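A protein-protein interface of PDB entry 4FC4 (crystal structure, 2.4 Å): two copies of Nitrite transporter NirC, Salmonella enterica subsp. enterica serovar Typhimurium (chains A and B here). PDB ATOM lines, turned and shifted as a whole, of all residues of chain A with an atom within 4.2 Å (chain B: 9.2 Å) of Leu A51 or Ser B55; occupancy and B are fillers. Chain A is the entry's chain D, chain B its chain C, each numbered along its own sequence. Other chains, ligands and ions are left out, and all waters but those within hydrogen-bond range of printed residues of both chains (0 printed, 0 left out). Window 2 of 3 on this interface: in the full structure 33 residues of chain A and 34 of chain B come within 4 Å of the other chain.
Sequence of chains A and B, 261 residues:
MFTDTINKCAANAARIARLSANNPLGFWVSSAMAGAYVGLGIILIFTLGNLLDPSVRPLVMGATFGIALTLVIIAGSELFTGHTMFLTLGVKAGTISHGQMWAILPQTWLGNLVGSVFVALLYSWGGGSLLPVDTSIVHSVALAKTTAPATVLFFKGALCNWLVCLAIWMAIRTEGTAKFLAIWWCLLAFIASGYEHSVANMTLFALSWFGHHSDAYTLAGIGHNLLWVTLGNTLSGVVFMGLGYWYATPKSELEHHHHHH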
ATOM      1  N   THR A  47      -3.368  11.218   6.030  1.00  0.00           N
ATOM      2  CA  THR A  47      -2.348  10.562   6.883  1.00  0.00           C
ATOM      3  C   THR A  47      -1.155  11.462   7.070  1.00  0.00           C
ATOM      4  O   THR A  47      -0.633  11.618   8.195  1.00  0.00           O
ATOM      5  CB  THR A  47      -1.876   9.201   6.330  1.00  0.00           C
ATOM      6  OG1 THR A  47      -3.034   8.396   6.036  1.00  0.00           O
ATOM      7  CG2 THR A  47      -0.970   8.437   7.326  1.00  0.00           C
ATOM      8  N   LEU A  48      -0.706  12.058   5.971  1.00  0.00           N
ATOM      9  CA  LEU A  48       0.516  12.855   6.035  1.00  0.00           C
ATOM     10  C   LEU A  48       0.170  14.188   6.715  1.00  0.00           C
ATOM     11  O   LEU A  48       0.857  14.590   7.630  1.00  0.00           O
ATOM     12  CB  LEU A  48       1.162  13.061   4.655  1.00  0.00           C
ATOM     13  CG  LEU A  48       1.655  11.878   3.827  1.00  0.00           C
ATOM     14  CD1 LEU A  48       1.968  12.301   2.368  1.00  0.00           C
ATOM     15  CD2 LEU A  48       2.857  11.227   4.518  1.00  0.00           C
ATOM     16  N   GLY A  49      -0.909  14.851   6.297  1.00  0.00           N
ATOM     17  CA  GLY A  49      -1.300  16.131   6.935  1.00  0.00           C
ATOM     18  C   GLY A  49      -1.481  16.050   8.449  1.00  0.00           C
ATOM     19  O   GLY A  49      -1.166  17.008   9.181  1.00  0.00           O
ATOM     20  N   ASN A  50      -2.027  14.923   8.919  1.00  0.00           N
ATOM     21  CA  ASN A  50      -2.411  14.766  10.337  1.00  0.00           C
ATOM     22  C   ASN A  50      -1.229  14.827  11.259  1.00  0.00           C
ATOM     23  O   ASN A  50      -1.368  15.213  12.398  1.00  0.00           O
ATOM     24  CB  ASN A  50      -3.139  13.448  10.558  1.00  0.00           C
ATOM     25  CG  ASN A  50      -3.915  13.409  11.880  1.00  0.00           C
ATOM     26  OD1 ASN A  50      -4.662  14.342  12.235  1.00  0.00           O
ATOM     27  ND2 ASN A  50      -3.752  12.316  12.597  1.00  0.00           N
ATOM     28  N   LEU A  51      -0.059  14.469  10.744  1.00  0.00           N
ATOM     29  CA  LEU A  51       1.148  14.449  11.553  1.00  0.00           C
ATOM     30  C   LEU A  51       1.921  15.791  11.523  1.00  0.00           C
ATOM     31  O   LEU A  51       2.870  16.015  12.306  1.00  0.00           O
ATOM     32  CB  LEU A  51       2.025  13.243  11.142  1.00  0.00           C
ATOM     33  CG  LEU A  51       1.538  11.896  11.782  1.00  0.00           C
ATOM     34  CD1 LEU A  51       2.513  10.767  11.559  1.00  0.00           C
ATOM     35  CD2 LEU A  51       1.227  11.916  13.271  1.00  0.00           C
ATOM     36  N   LEU A  52       1.501  16.702  10.645  1.00  0.00           N
ATOM     37  CA  LEU A  52       2.329  17.861  10.347  1.00  0.00           C
ATOM     38  C   LEU A  52       1.791  19.145  10.917  1.00  0.00           C
ATOM     39  O   LEU A  52       0.602  19.278  11.128  1.00  0.00           O
ATOM     40  CB  LEU A  52       2.487  18.010   8.846  1.00  0.00           C
ATOM     41  CG  LEU A  52       3.370  16.972   8.158  1.00  0.00           C
ATOM     42  CD1 LEU A  52       3.473  17.320   6.676  1.00  0.00           C
ATOM     43  CD2 LEU A  52       4.743  16.857   8.798  1.00  0.00           C
ATOM     44  N   GLY B  49      14.277   6.013   8.052  1.00  0.00           N
ATOM     45  CA  GLY B  49      13.243   6.236   9.047  1.00  0.00           C
ATOM     46  C   GLY B  49      13.782   6.310  10.465  1.00  0.00           C
ATOM     47  O   GLY B  49      13.283   7.057  11.315  1.00  0.00           O
ATOM     48  N   LEU B  52      14.593   9.772  11.809  1.00  0.00           N
ATOM     49  CA  LEU B  52      13.606  10.835  11.746  1.00  0.00           C
ATOM     50  C   LEU B  52      12.534  10.770  12.869  1.00  0.00           C
ATOM     51  O   LEU B  52      12.194   9.678  13.378  1.00  0.00           O
ATOM     52  CB  LEU B  52      12.955  10.802  10.360  1.00  0.00           C
ATOM     53  CG  LEU B  52      13.923  11.160   9.215  1.00  0.00           C
ATOM     54  CD1 LEU B  52      13.484  10.504   7.910  1.00  0.00           C
ATOM     55  CD2 LEU B  52      14.137  12.672   9.020  1.00  0.00           C
ATOM     56  N   ASP B  53      12.027  11.952  13.227  1.00  0.00           N
ATOM     57  CA  ASP B  53      10.793  12.139  13.988  1.00  0.00           C
ATOM     58  C   ASP B  53       9.723  11.277  13.413  1.00  0.00           C
ATOM     59  O   ASP B  53       9.584  11.231  12.208  1.00  0.00           O
ATOM     60  CB  ASP B  53      10.211  13.530  13.756  1.00  0.00           C
ATOM     61  CG  ASP B  53      10.718  14.494  14.666  1.00  0.00           C
ATOM     62  OD1 ASP B  53      11.677  14.138  15.398  1.00  0.00           O
ATOM     63  OD2 ASP B  53      10.141  15.613  14.662  1.00  0.00           O
ATOM     64  N   PRO B  54       8.909  10.674  14.288  1.00  0.00           N
ATOM     65  CA  PRO B  54       7.676  10.065  13.853  1.00  0.00           C
ATOM     66  C   PRO B  54       6.894  10.858  12.841  1.00  0.00           C
ATOM     67  O   PRO B  54       6.297  10.250  11.976  1.00  0.00           O
ATOM     68  CB  PRO B  54       6.867   9.939  15.156  1.00  0.00           C
ATOM     69  CG  PRO B  54       7.940   9.650  16.173  1.00  0.00           C
ATOM     70  CD  PRO B  54       9.150  10.449  15.740  1.00  0.00           C
ATOM     71  N   SER B  55       6.837  12.171  12.960  1.00  0.00           N
ATOM     72  CA  SER B  55       5.873  12.921  12.140  1.00  0.00           C
ATOM     73  C   SER B  55       6.310  13.054  10.653  1.00  0.00           C
ATOM     74  O   SER B  55       5.481  13.451   9.816  1.00  0.00           O
ATOM     75  CB  SER B  55       5.654  14.319  12.729  1.00  0.00           C
ATOM     76  OG  SER B  55       6.811  15.135  12.562  1.00  0.00           O
ATOM     77  N   VAL B  56       7.606  12.765  10.362  1.00  0.00           N
ATOM     78  CA  VAL B  56       8.144  12.767   8.998  1.00  0.00           C
ATOM     79  C   VAL B  56       8.577  11.386   8.499  1.00  0.00           C
ATOM     80  O   VAL B  56       8.933  11.248   7.323  1.00  0.00           O
ATOM     81  CB  VAL B  56       9.255  13.876   8.748  1.00  0.00           C
ATOM     82  CG1 VAL B  56       8.727  15.265   9.052  1.00  0.00           C
ATOM     83  CG2 VAL B  56      10.543  13.660   9.554  1.00  0.00           C
ATOM     84  N   ARG B  57       8.550  10.363   9.369  1.00  0.00           N
ATOM     85  CA  ARG B  57       8.766   8.960   8.920  1.00  0.00           C
ATOM     86  C   ARG B  57       7.906   8.503   7.745  1.00  0.00           C
ATOM     87  O   ARG B  57       8.421   8.014   6.750  1.00  0.00           O
ATOM     88  CB  ARG B  57       8.556   7.957  10.060  1.00  0.00           C
ATOM     89  CG  ARG B  57       9.851   7.709  10.765  1.00  0.00           C
ATOM     90  CD  ARG B  57       9.754   6.748  11.893  1.00  0.00           C
ATOM     91  NE  ARG B  57      10.655   7.273  12.906  1.00  0.00           N
ATOM     92  CZ  ARG B  57      10.548   7.011  14.200  1.00  0.00           C
ATOM     93  NH1 ARG B  57      11.388   7.563  15.031  1.00  0.00           N
ATOM     94  NH2 ARG B  57       9.602   6.222  14.651  1.00  0.00           N
ATOM     95  N   PRO B  58       6.569   8.654   7.858  1.00  0.00           N
ATOM     96  CA  PRO B  58       5.746   8.159   6.747  1.00  0.00           C
ATOM     97  C   PRO B  58       6.068   8.802   5.359  1.00  0.00           C
ATOM     98  O   PRO B  58       6.165   8.075   4.340  1.00  0.00           O
ATOM     99  CB  PRO B  58       4.309   8.465   7.233  1.00  0.00           C
ATOM    100  CG  PRO B  58       4.408   8.318   8.724  1.00  0.00           C
ATOM    101  CD  PRO B  58       5.757   8.916   9.067  1.00  0.00           C
ATOM    102  N   LEU B  59       6.262  10.113   5.345  1.00  0.00           N
ATOM    103  CA  LEU B  59       6.581  10.858   4.157  1.00  0.00           C
ATOM    104  C   LEU B  59       7.940  10.413   3.543  1.00  0.00           C
ATOM    105  O   LEU B  59       8.022  10.082   2.358  1.00  0.00           O
ATOM    106  CB  LEU B  59       6.566  12.373   4.470  1.00  0.00           C
ATOM    107  CG  LEU B  59       7.092  13.303   3.376  1.00  0.00           C
ATOM    108  CD1 LEU B  59       6.118  13.342   2.185  1.00  0.00           C
ATOM    109  CD2 LEU B  59       7.429  14.681   3.973  1.00  0.00           C
ATOM    110  N   VAL B  60       8.978  10.402   4.351  1.00  0.00           N
ATOM    111  CA  VAL B  60      10.322  10.101   3.832  1.00  0.00           C
ATOM    112  C   VAL B  60      10.474   8.593   3.513  1.00  0.00           C
ATOM    113  O   VAL B  60      10.985   8.221   2.443  1.00  0.00           O
ATOM    114  CB  VAL B  60      11.459  10.605   4.791  1.00  0.00           C
ATOM    115  CG1 VAL B  60      12.794  10.176   4.265  1.00  0.00           C
ATOM    116  CG2 VAL B  60      11.441  12.125   4.966  1.00  0.00           C
ATOM    117  N   MET B  61      10.035   7.727   4.432  1.00  0.00           N
ATOM    118  CA  MET B  61       9.910   6.272   4.091  1.00  0.00           C
ATOM    119  C   MET B  61       9.027   5.986   2.864  1.00  0.00           C
ATOM    120  O   MET B  61       9.396   5.204   2.027  1.00  0.00           O
ATOM    121  CB  MET B  61       9.478   5.445   5.291  1.00  0.00           C
ATOM    122  CG  MET B  61      10.498   5.516   6.420  1.00  0.00           C
ATOM    123  SD  MET B  61       9.999   4.628   7.927  1.00  0.00           S
ATOM    124  CE  MET B  61      10.171   2.871   7.475  1.00  0.00           C
ATOM    125  N   ALA B 192       3.119   5.226   3.369  1.00  0.00           N
ATOM    126  CA  ALA B 192       2.658   6.341   4.192  1.00  0.00           C
ATOM    127  C   ALA B 192       1.253   6.129   4.786  1.00  0.00           C
ATOM    128  O   ALA B 192       0.969   6.593   5.893  1.00  0.00           O
ATOM    129  CB  ALA B 192       2.700   7.632   3.374  1.00  0.00           C
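Thr A47 touches Ala B192 (CG2 to O, 3.0 Å).
Leu B59 touches Leu A48.
CD2 of Leu A48 touches CB of Ala B192 (3.8 Å).
O of Pro B54 touches CD1 of Leu A51, 3.8 Å away.
O of Leu A51 touches CB of Ser B55, at 3.3 Å.
CD2 of Leu A52 touches O of Ser B55, 3.6 Å away.
Leu A51 touches just these residues of chain B: Pro B54 (3.8 Å) and Ser B55 (3.3 Å).
Ser B55 touches just these residues of chain A: Leu A51 and Leu A52.
No residue of chain B comes within 4 Å of Gly A49.
No residue of chain B comes within 4 Å of Asn A50.
Printed residues of chain A within 4 Å of Leu B59: Leu A48 (3.7 Å).
Printed residues of chain B within 4 Å of Leu A52: Ser B55.
Printed residues of chain A within 4 Å of Pro B54: Leu A51.
Gly B49 touches none of the printed residues of chain A.
The nearest residue of chain B that does not touch Leu A51 is Pro B58 (4.2 Å).
Along chain A the printed residues that touch a printed residue of chain B span positions 47 to 52.
Of the 12 printed residues of chain B, 4 touch a printed residue of chain A.
Along chain B the printed residues that touch a printed residue of chain A span positions 54 to 192.
Among the printed residues, no Asp or Glu carboxylate lies within 4 Å of a Lys or Arg side-chain nitrogen of the other chain.
Positions printed for both chains: 49 and 52.
Of the 6 pairs that touch across the chains among the printed residues, none has its exchanged pair printed and touching as well.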
